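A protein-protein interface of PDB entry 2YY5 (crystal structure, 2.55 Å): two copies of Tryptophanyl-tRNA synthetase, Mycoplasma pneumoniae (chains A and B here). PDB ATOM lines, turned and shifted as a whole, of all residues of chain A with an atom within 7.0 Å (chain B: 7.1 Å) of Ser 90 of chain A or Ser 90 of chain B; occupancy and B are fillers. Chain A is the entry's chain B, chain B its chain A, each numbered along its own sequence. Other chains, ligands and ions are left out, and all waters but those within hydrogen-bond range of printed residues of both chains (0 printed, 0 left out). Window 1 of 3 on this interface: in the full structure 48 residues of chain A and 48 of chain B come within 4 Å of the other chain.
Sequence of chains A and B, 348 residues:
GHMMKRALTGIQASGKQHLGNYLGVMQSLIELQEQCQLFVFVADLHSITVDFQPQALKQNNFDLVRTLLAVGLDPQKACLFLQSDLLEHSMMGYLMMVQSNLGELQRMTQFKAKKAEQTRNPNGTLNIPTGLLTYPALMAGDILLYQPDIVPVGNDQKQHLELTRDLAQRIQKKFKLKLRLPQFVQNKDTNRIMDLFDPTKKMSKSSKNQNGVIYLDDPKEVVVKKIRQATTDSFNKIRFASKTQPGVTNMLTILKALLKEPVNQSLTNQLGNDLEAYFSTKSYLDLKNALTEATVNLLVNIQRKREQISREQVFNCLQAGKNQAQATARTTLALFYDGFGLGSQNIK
O of Leu 45 of chain B is in hydrogen-bond range of OH of Tyr 94 of chain A.
The side-chain hydroxyl of Ser 90 of chain A is in hydrogen-bond range of the side-chain hydroxyl of Ser 90 of chain B (2.7 Å).
The side-chain hydroxyl (OG) of Ser 90 of chain B is in hydrogen-bond range of the backbone NH (N) of Met 91 of chain A (3.1 Å).
OG of Ser 90 of chain A lies within hydrogen-bond range of N of Met 91 of chain B (3.2 Å).
The backbone carbonyl oxygen of Leu 45 of chain A lies within hydrogen-bond range of the side-chain hydroxyl of Tyr 94 of chain B, 2.5 Å away.
The side-chain sulfur (SD) of Met 97 of chain A lies close to the side-chain sulfur (SD) of Met 97 of chain B (3.7 Å).
The side-chain amide oxygen (OE1) of Gln 83 of chain B sits at hydrogen-bond distance from the backbone NH (N) of Leu 45 of chain B (2.9 Å).
OG of Ser 90 of chain B is in hydrogen-bond range of O of Leu 87 of chain B (2.8 Å).
The side-chain sulfur (SD) of Met 91 of chain B lies close to the side-chain hydroxyl (OH) of Tyr 337 of chain B (3.8 Å).
N of Leu 45 of chain A is in hydrogen-bond range of OE1 of Gln 83 of chain A (3.0 Å).
The side-chain hydroxyl of Ser 90 of chain A lies within hydrogen-bond range of the backbone carbonyl oxygen of Leu 87 of chain A (2.8 Å).
OH of Tyr 337 of chain A lies close to SD of Met 91 of chain A, at 3.7 Å.
Leu 45 of chain A touches Met 91 of chain B.
Leu 87 of chain A touches Leu 87 of chain B.
Leu 87 of chain A touches Glu 88 of chain B (CD2 to OE1, 3.9 Å).
Leu 87 of chain A touches Ser 90 of chain B.
Leu 87 of chain A touches Tyr 337 of chain B.
Leu 87 of chain B touches Glu 88 of chain A (CD2 to OE1, 3.9 Å).
Leu 87 of chain B touches Ser 90 of chain A.
CD1 of Leu 138 of chain B touches OH of Tyr 94 of chain A (3.3 Å).
Tyr 94 of chain B touches Leu 138 of chain A.
OH of Tyr 337 of chain A touches CD1 of Leu 87 of chain B (3.8 Å).
Ser 90 of chain A touches just these residues of chain B: Leu 87 (3.98 Å), Ser 90 (2.7 Å) and Met 91 (3.2 Å).
Printed residues of chain A within 4 Å of Ser 90 of chain B: Leu 87, Ser 90 and Met 91.
Of the printed residues of chain A, Met 91 of chain B touches Leu 45 (3.998 Å) and Ser 90 (3.2 Å).
Of the printed residues of chain A, Met 97 of chain B touches Met 97 (3.7 Å).
The nearest residue of chain B that does not touch Ser 90 of chain A is Tyr 94 of chain B (4.5 Å).
Of the 17 printed residues of chain A, 9 touch a printed residue of chain B.
Hydrophobic or aromatic side chains of chain B that line the printed part of chain A: Leu 45, Leu 87, Met 91, Tyr 94, Met 97, Leu 138 and Tyr 337.
Among the printed residues, 17 pairs touch across the chains.
Among the printed residues, no Asp or Glu carboxylate lies within 4 Å of a Lys or Arg side-chain nitrogen of the other chain.
Leu 45 of chain A touches Tyr 94 of chain B, and with the chains exchanged Tyr 94 of chain A touches Leu 45 of chain B.
Leu 87 of chain A touches Glu 88 of chain B, and with the chains exchanged Glu 88 of chain A touches Leu 87 of chain B.
Leu 87 of chain A touches Ser 90 of chain B, and with the chains exchanged Ser 90 of chain A touches Leu 87 of chain B.
Leu 87 of chain A touches Tyr 337 of chain B, and with the chains exchanged Tyr 337 of chain A touches Leu 87 of chain B.
17 positions are printed for both chains.
Of the 17 pairs that touch across the chains among the printed residues, 17 have their exchanged pair printed and touching as well.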
ATOM      1  N   LEU A  45       2.703 -17.290 -34.228  1.00  0.00           N
ATOM      2  CA  LEU A  45       1.732 -17.435 -33.146  1.00  0.00           C
ATOM      3  C   LEU A  45       1.992 -16.321 -32.130  1.00  0.00           C
ATOM      4  O   LEU A  45       1.130 -15.989 -31.320  1.00  0.00           O
ATOM      5  CB  LEU A  45       1.856 -18.816 -32.487  1.00  0.00           C
ATOM      6  CG  LEU A  45       1.465 -19.996 -33.391  1.00  0.00           C
ATOM      7  CD1 LEU A  45       1.657 -21.292 -32.643  1.00  0.00           C
ATOM      8  CD2 LEU A  45       0.017 -19.864 -33.848  1.00  0.00           C
ATOM      9  N   GLN A  83       5.792 -21.865 -37.280  1.00  0.00           N
ATOM     10  CA  GLN A  83       5.204 -22.237 -35.997  1.00  0.00           C
ATOM     11  C   GLN A  83       3.748 -22.719 -36.063  1.00  0.00           C
ATOM     12  O   GLN A  83       3.407 -23.765 -35.516  1.00  0.00           O
ATOM     13  CB  GLN A  83       5.326 -21.054 -35.024  1.00  0.00           C
ATOM     14  CG  GLN A  83       4.798 -21.313 -33.619  1.00  0.00           C
ATOM     15  CD  GLN A  83       4.969 -20.109 -32.712  1.00  0.00           C
ATOM     16  OE1 GLN A  83       4.988 -18.973 -33.176  1.00  0.00           O
ATOM     17  NE2 GLN A  83       5.074 -20.351 -31.412  1.00  0.00           N
ATOM     18  N   LEU A  86       2.461 -26.378 -36.919  1.00  0.00           N
ATOM     19  CA  LEU A  86       2.495 -27.440 -35.924  1.00  0.00           C
ATOM     20  C   LEU A  86       1.571 -27.227 -34.718  1.00  0.00           C
ATOM     21  O   LEU A  86       1.867 -26.444 -33.821  1.00  0.00           O
ATOM     22  CB  LEU A  86       3.927 -27.644 -35.412  1.00  0.00           C
ATOM     23  CG  LEU A  86       4.933 -28.310 -36.348  1.00  0.00           C
ATOM     24  CD1 LEU A  86       5.199 -27.402 -37.540  1.00  0.00           C
ATOM     25  CD2 LEU A  86       6.226 -28.598 -35.587  1.00  0.00           C
ATOM     26  N   LEU A  87       0.455 -27.938 -34.688  1.00  0.00           N
ATOM     27  CA  LEU A  87      -0.448 -27.837 -33.551  1.00  0.00           C
ATOM     28  C   LEU A  87       0.292 -28.174 -32.250  1.00  0.00           C
ATOM     29  O   LEU A  87      -0.159 -27.797 -31.159  1.00  0.00           O
ATOM     30  CB  LEU A  87      -1.631 -28.795 -33.736  1.00  0.00           C
ATOM     31  CG  LEU A  87      -2.849 -28.290 -34.519  1.00  0.00           C
ATOM     32  CD1 LEU A  87      -2.475 -27.132 -35.418  1.00  0.00           C
ATOM     33  CD2 LEU A  87      -3.427 -29.433 -35.309  1.00  0.00           C
ATOM     34  N   GLU A  88       1.419 -28.885 -32.358  1.00  0.00           N
ATOM     35  CA  GLU A  88       2.197 -29.257 -31.176  1.00  0.00           C
ATOM     36  C   GLU A  88       2.649 -28.031 -30.402  1.00  0.00           C
ATOM     37  O   GLU A  88       2.864 -28.096 -29.199  1.00  0.00           O
ATOM     38  CB  GLU A  88       3.437 -30.082 -31.548  1.00  0.00           C
ATOM     39  CG  GLU A  88       3.181 -31.542 -31.911  1.00  0.00           C
ATOM     40  CD  GLU A  88       2.614 -31.684 -33.303  1.00  0.00           C
ATOM     41  OE1 GLU A  88       2.348 -32.823 -33.740  1.00  0.00           O
ATOM     42  OE2 GLU A  88       2.439 -30.644 -33.968  1.00  0.00           O
ATOM     43  N   HIS A  89       2.797 -26.909 -31.093  1.00  0.00           N
ATOM     44  CA  HIS A  89       3.228 -25.690 -30.434  1.00  0.00           C
ATOM     45  C   HIS A  89       2.151 -25.141 -29.515  1.00  0.00           C
ATOM     46  O   HIS A  89       2.424 -24.841 -28.360  1.00  0.00           O
ATOM     47  CB  HIS A  89       3.665 -24.663 -31.476  1.00  0.00           C
ATOM     48  CG  HIS A  89       5.061 -24.886 -31.966  1.00  0.00           C
ATOM     49  ND1 HIS A  89       6.161 -24.341 -31.341  1.00  0.00           N
ATOM     50  CD2 HIS A  89       5.545 -25.681 -32.951  1.00  0.00           C
ATOM     51  CE1 HIS A  89       7.264 -24.795 -31.918  1.00  0.00           C
ATOM     52  NE2 HIS A  89       6.915 -25.611 -32.896  1.00  0.00           N
ATOM     53  N   SER A  90       0.925 -25.046 -30.010  1.00  0.00           N
ATOM     54  CA  SER A  90      -0.169 -24.544 -29.193  1.00  0.00           C
ATOM     55  C   SER A  90      -0.374 -25.456 -27.985  1.00  0.00           C
ATOM     56  O   SER A  90      -0.628 -24.986 -26.874  1.00  0.00           O
ATOM     57  CB  SER A  90      -1.465 -24.475 -30.011  1.00  0.00           C
ATOM     58  OG  SER A  90      -1.948 -25.768 -30.339  1.00  0.00           O
ATOM     59  N   MET A  91      -0.248 -26.761 -28.202  1.00  0.00           N
ATOM     60  CA  MET A  91      -0.451 -27.708 -27.118  1.00  0.00           C
ATOM     61  C   MET A  91       0.626 -27.627 -26.059  1.00  0.00           C
ATOM     62  O   MET A  91       0.325 -27.586 -24.871  1.00  0.00           O
ATOM     63  CB  MET A  91      -0.548 -29.133 -27.658  1.00  0.00           C
ATOM     64  CG  MET A  91      -0.848 -30.179 -26.591  1.00  0.00           C
ATOM     65  SD  MET A  91      -2.169 -29.701 -25.449  1.00  0.00           S
ATOM     66  CE  MET A  91      -3.596 -30.351 -26.259  1.00  0.00           C
ATOM     67  N   MET A  92       1.884 -27.607 -26.478  1.00  0.00           N
ATOM     68  CA  MET A  92       2.974 -27.530 -25.519  1.00  0.00           C
ATOM     69  C   MET A  92       2.906 -26.184 -24.805  1.00  0.00           C
ATOM     70  O   MET A  92       3.121 -26.101 -23.594  1.00  0.00           O
ATOM     71  CB  MET A  92       4.328 -27.701 -26.229  1.00  0.00           C
ATOM     72  CG  MET A  92       5.548 -27.664 -25.300  1.00  0.00           C
ATOM     73  SD  MET A  92       5.543 -28.921 -23.977  1.00  0.00           S
ATOM     74  CE  MET A  92       6.483 -30.208 -24.743  1.00  0.00           C
ATOM     75  N   GLY A  93       2.582 -25.135 -25.559  1.00  0.00           N
ATOM     76  CA  GLY A  93       2.487 -23.800 -24.993  1.00  0.00           C
ATOM     77  C   GLY A  93       1.430 -23.752 -23.913  1.00  0.00           C
ATOM     78  O   GLY A  93       1.562 -23.020 -22.921  1.00  0.00           O
ATOM     79  N   TYR A  94       0.382 -24.549 -24.108  1.00  0.00           N
ATOM     80  CA  TYR A  94      -0.716 -24.634 -23.155  1.00  0.00           C
ATOM     81  C   TYR A  94      -0.283 -25.322 -21.866  1.00  0.00           C
ATOM     82  O   TYR A  94      -0.652 -24.884 -20.773  1.00  0.00           O
ATOM     83  CB  TYR A  94      -1.909 -25.380 -23.769  1.00  0.00           C
ATOM     84  CG  TYR A  94      -3.110 -25.473 -22.844  1.00  0.00           C
ATOM     85  CD1 TYR A  94      -3.271 -26.549 -21.967  1.00  0.00           C
ATOM     86  CD2 TYR A  94      -4.055 -24.457 -22.814  1.00  0.00           C
ATOM     87  CE1 TYR A  94      -4.340 -26.597 -21.086  1.00  0.00           C
ATOM     88  CE2 TYR A  94      -5.122 -24.495 -21.944  1.00  0.00           C
ATOM     89  CZ  TYR A  94      -5.266 -25.557 -21.080  1.00  0.00           C
ATOM     90  OH  TYR A  94      -6.328 -25.541 -20.209  1.00  0.00           O
ATOM     91  N   LEU A  95       0.499 -26.393 -21.980  1.00  0.00           N
ATOM     92  CA  LEU A  95       0.954 -27.097 -20.781  1.00  0.00           C
ATOM     93  C   LEU A  95       1.818 -26.164 -19.953  1.00  0.00           C
ATOM     94  O   LEU A  95       1.741 -26.150 -18.729  1.00  0.00           O
ATOM     95  CB  LEU A  95       1.753 -28.352 -21.144  1.00  0.00           C
ATOM     96  CG  LEU A  95       1.028 -29.418 -21.957  1.00  0.00           C
ATOM     97  CD1 LEU A  95       1.906 -30.642 -22.061  1.00  0.00           C
ATOM     98  CD2 LEU A  95      -0.296 -29.763 -21.296  1.00  0.00           C
ATOM     99  N   MET A  97       1.691 -22.811 -19.995  1.00  0.00           N
ATOM    100  CA  MET A  97       0.794 -21.791 -19.447  1.00  0.00           C
ATOM    101  C   MET A  97       0.059 -22.229 -18.169  1.00  0.00           C
ATOM    102  O   MET A  97      -0.003 -21.478 -17.193  1.00  0.00           O
ATOM    103  CB  MET A  97      -0.230 -21.361 -20.511  1.00  0.00           C
ATOM    104  CG  MET A  97      -1.236 -20.307 -20.036  1.00  0.00           C
ATOM    105  SD  MET A  97      -2.368 -19.715 -21.312  1.00  0.00           S
ATOM    106  CE  MET A  97      -3.291 -21.280 -21.729  1.00  0.00           C
ATOM    107  N   LEU A 138       4.353 -19.500 -24.186  1.00  0.00           N
ATOM    108  CA  LEU A 138       4.325 -20.116 -25.507  1.00  0.00           C
ATOM    109  C   LEU A 138       5.785 -20.313 -25.895  1.00  0.00           C
ATOM    110  O   LEU A 138       6.167 -21.350 -26.433  1.00  0.00           O
ATOM    111  CB  LEU A 138       3.679 -19.184 -26.533  1.00  0.00           C
ATOM    112  CG  LEU A 138       2.800 -19.805 -27.625  1.00  0.00           C
ATOM    113  CD1 LEU A 138       2.837 -18.900 -28.846  1.00  0.00           C
ATOM    114  CD2 LEU A 138       3.263 -21.216 -27.980  1.00  0.00           C
ATOM    115  N   ASP A 142       7.858 -23.497 -27.056  1.00  0.00           N
ATOM    116  CA  ASP A 142       8.522 -23.585 -28.354  1.00  0.00           C
ATOM    117  C   ASP A 142       9.924 -24.143 -28.152  1.00  0.00           C
ATOM    118  O   ASP A 142      10.405 -24.933 -28.957  1.00  0.00           O
ATOM    119  CB  ASP A 142       8.632 -22.209 -29.027  1.00  0.00           C
ATOM    120  CG  ASP A 142       7.276 -21.541 -29.263  1.00  0.00           C
ATOM    121  OD1 ASP A 142       6.305 -22.220 -29.679  1.00  0.00           O
ATOM    122  OD2 ASP A 142       7.198 -20.313 -29.044  1.00  0.00           O
ATOM    123  N   LEU A 145       9.929 -28.047 -26.771  1.00  0.00           N
ATOM    124  CA  LEU A 145       9.410 -29.032 -27.715  1.00  0.00           C
ATOM    125  C   LEU A 145      10.550 -29.724 -28.459  1.00  0.00           C
ATOM    126  O   LEU A 145      10.427 -30.874 -28.877  1.00  0.00           O
ATOM    127  CB  LEU A 145       8.502 -28.359 -28.744  1.00  0.00           C
ATOM    128  CG  LEU A 145       7.010 -28.680 -28.734  1.00  0.00           C
ATOM    129  CD1 LEU A 145       6.326 -27.894 -29.860  1.00  0.00           C
ATOM    130  CD2 LEU A 145       6.803 -30.183 -28.898  1.00  0.00           C
ATOM    131  N   TYR A 337       2.979 -35.935 -22.428  1.00  0.00           N
ATOM    132  CA  TYR A 337       1.641 -36.465 -22.239  1.00  0.00           C
ATOM    133  C   TYR A 337       1.714 -37.580 -21.216  1.00  0.00           C
ATOM    134  O   TYR A 337       0.878 -37.657 -20.322  1.00  0.00           O
ATOM    135  CB  TYR A 337       1.063 -36.983 -23.561  1.00  0.00           C
ATOM    136  CG  TYR A 337       0.071 -36.027 -24.192  1.00  0.00           C
ATOM    137  CD1 TYR A 337       0.368 -34.667 -24.318  1.00  0.00           C
ATOM    138  CD2 TYR A 337      -1.162 -36.475 -24.661  1.00  0.00           C
ATOM    139  CE1 TYR A 337      -0.539 -33.779 -24.889  1.00  0.00           C
ATOM    140  CE2 TYR A 337      -2.075 -35.590 -25.238  1.00  0.00           C
ATOM    141  CZ  TYR A 337      -1.753 -34.244 -25.347  1.00  0.00           C
ATOM    142  OH  TYR A 337      -2.641 -33.365 -25.917  1.00  0.00           O
ATOM    143  N   LEU B  45      -8.260 -30.839 -20.348  1.00  0.00           N
ATOM    144  CA  LEU B  45      -7.391 -29.683 -20.539  1.00  0.00           C
ATOM    145  C   LEU B  45      -7.778 -28.650 -19.490  1.00  0.00           C
ATOM    146  O   LEU B  45      -6.929 -27.885 -19.020  1.00  0.00           O
ATOM    147  CB  LEU B  45      -7.553 -29.093 -21.940  1.00  0.00           C
ATOM    148  CG  LEU B  45      -7.000 -29.959 -23.074  1.00  0.00           C
ATOM    149  CD1 LEU B  45      -7.257 -29.265 -24.412  1.00  0.00           C
ATOM    150  CD2 LEU B  45      -5.495 -30.207 -22.859  1.00  0.00           C
ATOM    151  N   GLN B  83     -10.769 -34.412 -24.817  1.00  0.00           N
ATOM    152  CA  GLN B  83     -10.180 -33.275 -25.525  1.00  0.00           C
ATOM    153  C   GLN B  83      -8.656 -33.241 -25.628  1.00  0.00           C
ATOM    154  O   GLN B  83      -8.124 -32.649 -26.557  1.00  0.00           O
ATOM    155  CB  GLN B  83     -10.676 -31.943 -24.957  1.00  0.00           C
ATOM    156  CG  GLN B  83     -10.277 -31.660 -23.544  1.00  0.00           C
ATOM    157  CD  GLN B  83     -10.412 -30.189 -23.186  1.00  0.00           C
ATOM    158  OE1 GLN B  83     -10.341 -29.818 -22.018  1.00  0.00           O
ATOM    159  NE2 GLN B  83     -10.598 -29.345 -24.190  1.00  0.00           N
ATOM    160  N   LEU B  86      -7.051 -34.293 -28.937  1.00  0.00           N
ATOM    161  CA  LEU B  86      -7.062 -33.438 -30.120  1.00  0.00           C
ATOM    162  C   LEU B  86      -6.251 -32.170 -29.900  1.00  0.00           C
ATOM    163  O   LEU B  86      -6.575 -31.348 -29.045  1.00  0.00           O
ATOM    164  CB  LEU B  86      -8.477 -33.024 -30.511  1.00  0.00           C
ATOM    165  CG  LEU B  86      -9.572 -34.039 -30.815  1.00  0.00           C
ATOM    166  CD1 LEU B  86     -10.626 -33.321 -31.627  1.00  0.00           C
ATOM    167  CD2 LEU B  86      -9.039 -35.214 -31.591  1.00  0.00           C
ATOM    168  N   LEU B  87      -5.190 -32.021 -30.681  1.00  0.00           N
ATOM    169  CA  LEU B  87      -4.345 -30.847 -30.604  1.00  0.00           C
ATOM    170  C   LEU B  87      -5.129 -29.633 -31.092  1.00  0.00           C
ATOM    171  O   LEU B  87      -4.818 -28.494 -30.732  1.00  0.00           O
ATOM    172  CB  LEU B  87      -3.083 -31.062 -31.452  1.00  0.00           C
ATOM    173  CG  LEU B  87      -1.835 -31.596 -30.737  1.00  0.00           C
ATOM    174  CD1 LEU B  87      -2.207 -32.532 -29.622  1.00  0.00           C
ATOM    175  CD2 LEU B  87      -0.942 -32.267 -31.749  1.00  0.00           C
ATOM    176  N   GLU B  88      -6.157 -29.883 -31.902  1.00  0.00           N
ATOM    177  CA  GLU B  88      -6.993 -28.810 -32.426  1.00  0.00           C
ATOM    178  C   GLU B  88      -7.559 -27.953 -31.298  1.00  0.00           C
ATOM    179  O   GLU B  88      -7.712 -26.742 -31.458  1.00  0.00           O
ATOM    180  CB  GLU B  88      -8.148 -29.365 -33.263  1.00  0.00           C
ATOM    181  CG  GLU B  88      -7.754 -29.927 -34.627  1.00  0.00           C
ATOM    182  CD  GLU B  88      -7.090 -31.289 -34.541  1.00  0.00           C
ATOM    183  OE1 GLU B  88      -6.548 -31.752 -35.574  1.00  0.00           O
ATOM    184  OE2 GLU B  88      -7.110 -31.903 -33.449  1.00  0.00           O
ATOM    185  N   HIS B  89      -7.869 -28.570 -30.158  1.00  0.00           N
ATOM    186  CA  HIS B  89      -8.411 -27.809 -29.031  1.00  0.00           C
ATOM    187  C   HIS B  89      -7.455 -26.741 -28.511  1.00  0.00           C
ATOM    188  O   HIS B  89      -7.853 -25.589 -28.316  1.00  0.00           O
ATOM    189  CB  HIS B  89      -8.816 -28.748 -27.898  1.00  0.00           C
ATOM    190  CG  HIS B  89     -10.158 -29.370 -28.095  1.00  0.00           C
ATOM    191  ND1 HIS B  89     -11.318 -28.802 -27.614  1.00  0.00           N
ATOM    192  CD2 HIS B  89     -10.538 -30.467 -28.787  1.00  0.00           C
ATOM    193  CE1 HIS B  89     -12.356 -29.520 -28.003  1.00  0.00           C
ATOM    194  NE2 HIS B  89     -11.909 -30.537 -28.719  1.00  0.00           N
ATOM    195  N   SER B  90      -6.196 -27.119 -28.298  1.00  0.00           N
ATOM    196  CA  SER B  90      -5.199 -26.175 -27.814  1.00  0.00           C
ATOM    197  C   SER B  90      -4.979 -25.057 -28.821  1.00  0.00           C
ATOM    198  O   SER B  90      -4.714 -23.920 -28.432  1.00  0.00           O
ATOM    199  CB  SER B  90      -3.860 -26.875 -27.533  1.00  0.00           C
ATOM    200  OG  SER B  90      -3.283 -27.416 -28.710  1.00  0.00           O
ATOM    201  N   MET B  91      -5.095 -25.366 -30.113  1.00  0.00           N
ATOM    202  CA  MET B  91      -4.880 -24.333 -31.122  1.00  0.00           C
ATOM    203  C   MET B  91      -6.073 -23.413 -31.268  1.00  0.00           C
ATOM    204  O   MET B  91      -5.906 -22.193 -31.319  1.00  0.00           O
ATOM    205  CB  MET B  91      -4.520 -24.945 -32.480  1.00  0.00           C
ATOM    206  CG  MET B  91      -4.156 -23.912 -33.569  1.00  0.00           C
ATOM    207  SD  MET B  91      -2.787 -22.756 -33.192  1.00  0.00           S
ATOM    208  CE  MET B  91      -1.311 -23.880 -33.331  1.00  0.00           C
ATOM    209  N   MET B  92      -7.275 -23.987 -31.328  1.00  0.00           N
ATOM    210  CA  MET B  92      -8.484 -23.186 -31.454  1.00  0.00           C
ATOM    211  C   MET B  92      -8.597 -22.286 -30.230  1.00  0.00           C
ATOM    212  O   MET B  92      -8.991 -21.119 -30.334  1.00  0.00           O
ATOM    213  CB  MET B  92      -9.723 -24.077 -31.551  1.00  0.00           C
ATOM    214  CG  MET B  92     -11.022 -23.291 -31.669  1.00  0.00           C
ATOM    215  SD  MET B  92     -11.008 -22.133 -33.075  1.00  0.00           S
ATOM    216  CE  MET B  92     -11.788 -23.126 -34.321  1.00  0.00           C
ATOM    217  N   GLY B  93      -8.232 -22.841 -29.076  1.00  0.00           N
ATOM    218  CA  GLY B  93      -8.290 -22.094 -27.831  1.00  0.00           C
ATOM    219  C   GLY B  93      -7.248 -20.994 -27.762  1.00  0.00           C
ATOM    220  O   GLY B  93      -7.424 -19.996 -27.059  1.00  0.00           O
ATOM    221  N   TYR B  94      -6.150 -21.183 -28.483  1.00  0.00           N
ATOM    222  CA  TYR B  94      -5.094 -20.187 -28.518  1.00  0.00           C
ATOM    223  C   TYR B  94      -5.601 -18.999 -29.329  1.00  0.00           C
ATOM    224  O   TYR B  94      -5.348 -17.842 -28.987  1.00  0.00           O
ATOM    225  CB  TYR B  94      -3.821 -20.753 -29.171  1.00  0.00           C
ATOM    226  CG  TYR B  94      -2.700 -19.744 -29.223  1.00  0.00           C
ATOM    227  CD1 TYR B  94      -2.478 -18.954 -30.364  1.00  0.00           C
ATOM    228  CD2 TYR B  94      -1.911 -19.511 -28.093  1.00  0.00           C
ATOM    229  CE1 TYR B  94      -1.494 -17.946 -30.366  1.00  0.00           C
ATOM    230  CE2 TYR B  94      -0.940 -18.518 -28.084  1.00  0.00           C
ATOM    231  CZ  TYR B  94      -0.733 -17.739 -29.218  1.00  0.00           C
ATOM    232  OH  TYR B  94       0.232 -16.759 -29.172  1.00  0.00           O
ATOM    233  N   LEU B  95      -6.312 -19.292 -30.412  1.00  0.00           N
ATOM    234  CA  LEU B  95      -6.857 -18.239 -31.253  1.00  0.00           C
ATOM    235  C   LEU B  95      -7.914 -17.431 -30.493  1.00  0.00           C
ATOM    236  O   LEU B  95      -7.948 -16.207 -30.598  1.00  0.00           O
ATOM    237  CB  LEU B  95      -7.461 -18.826 -32.532  1.00  0.00           C
ATOM    238  CG  LEU B  95      -6.510 -19.632 -33.423  1.00  0.00           C
ATOM    239  CD1 LEU B  95      -7.203 -19.939 -34.757  1.00  0.00           C
ATOM    240  CD2 LEU B  95      -5.235 -18.857 -33.659  1.00  0.00           C
ATOM    241  N   MET B  97      -8.055 -17.104 -27.309  1.00  0.00           N
ATOM    242  CA  MET B  97      -7.308 -16.380 -26.290  1.00  0.00           C
ATOM    243  C   MET B  97      -6.676 -15.088 -26.803  1.00  0.00           C
ATOM    244  O   MET B  97      -6.848 -14.028 -26.193  1.00  0.00           O
ATOM    245  CB  MET B  97      -6.225 -17.280 -25.667  1.00  0.00           C
ATOM    246  CG  MET B  97      -5.320 -16.553 -24.672  1.00  0.00           C
ATOM    247  SD  MET B  97      -4.316 -17.622 -23.625  1.00  0.00           S
ATOM    248  CE  MET B  97      -3.090 -18.277 -24.848  1.00  0.00           C
ATOM    249  N   LEU B 138     -10.637 -20.940 -23.608  1.00  0.00           N
ATOM    250  CA  LEU B 138     -10.412 -22.294 -24.098  1.00  0.00           C
ATOM    251  C   LEU B 138     -11.789 -22.934 -24.250  1.00  0.00           C
ATOM    252  O   LEU B 138     -12.055 -23.659 -25.211  1.00  0.00           O
ATOM    253  CB  LEU B 138      -9.602 -23.096 -23.076  1.00  0.00           C
ATOM    254  CG  LEU B 138      -8.799 -24.339 -23.471  1.00  0.00           C
ATOM    255  CD1 LEU B 138      -8.834 -25.321 -22.310  1.00  0.00           C
ATOM    256  CD2 LEU B 138      -9.343 -24.981 -24.714  1.00  0.00           C
ATOM    257  N   ASP B 142     -13.422 -24.637 -27.425  1.00  0.00           N
ATOM    258  CA  ASP B 142     -13.945 -26.000 -27.481  1.00  0.00           C
ATOM    259  C   ASP B 142     -15.305 -26.002 -28.184  1.00  0.00           C
ATOM    260  O   ASP B 142     -15.622 -26.928 -28.932  1.00  0.00           O
ATOM    261  CB  ASP B 142     -14.124 -26.595 -26.073  1.00  0.00           C
ATOM    262  CG  ASP B 142     -12.831 -26.639 -25.267  1.00  0.00           C
ATOM    263  OD1 ASP B 142     -11.777 -27.045 -25.811  1.00  0.00           O
ATOM    264  OD2 ASP B 142     -12.883 -26.278 -24.068  1.00  0.00           O
ATOM    265  N   LEU B 145     -15.046 -24.892 -32.123  1.00  0.00           N
ATOM    266  CA  LEU B 145     -14.398 -25.918 -32.947  1.00  0.00           C
ATOM    267  C   LEU B 145     -15.380 -26.824 -33.691  1.00  0.00           C
ATOM    268  O   LEU B 145     -15.021 -27.433 -34.698  1.00  0.00           O
ATOM    269  CB  LEU B 145     -13.497 -26.817 -32.088  1.00  0.00           C
ATOM    270  CG  LEU B 145     -11.981 -26.833 -32.337  1.00  0.00           C
ATOM    271  CD1 LEU B 145     -11.341 -27.961 -31.504  1.00  0.00           C
ATOM    272  CD2 LEU B 145     -11.687 -27.013 -33.831  1.00  0.00           C
ATOM    273  N   TYR B 337      -7.930 -20.919 -40.002  1.00  0.00           N
ATOM    274  CA  TYR B 337      -6.565 -20.684 -40.428  1.00  0.00           C
ATOM    275  C   TYR B 337      -6.534 -19.746 -41.624  1.00  0.00           C
ATOM    276  O   TYR B 337      -5.822 -18.738 -41.605  1.00  0.00           O
ATOM    277  CB  TYR B 337      -5.888 -22.012 -40.764  1.00  0.00           C
ATOM    278  CG  TYR B 337      -4.924 -22.491 -39.699  1.00  0.00           C
ATOM    279  CD1 TYR B 337      -5.364 -22.812 -38.415  1.00  0.00           C
ATOM    280  CD2 TYR B 337      -3.559 -22.600 -39.973  1.00  0.00           C
ATOM    281  CE1 TYR B 337      -4.469 -23.228 -37.436  1.00  0.00           C
ATOM    282  CE2 TYR B 337      -2.662 -23.011 -39.004  1.00  0.00           C
ATOM    283  CZ  TYR B 337      -3.123 -23.323 -37.739  1.00  0.00           C
ATOM    284  OH  TYR B 337      -2.237 -23.734 -36.783  1.00  0.00           O
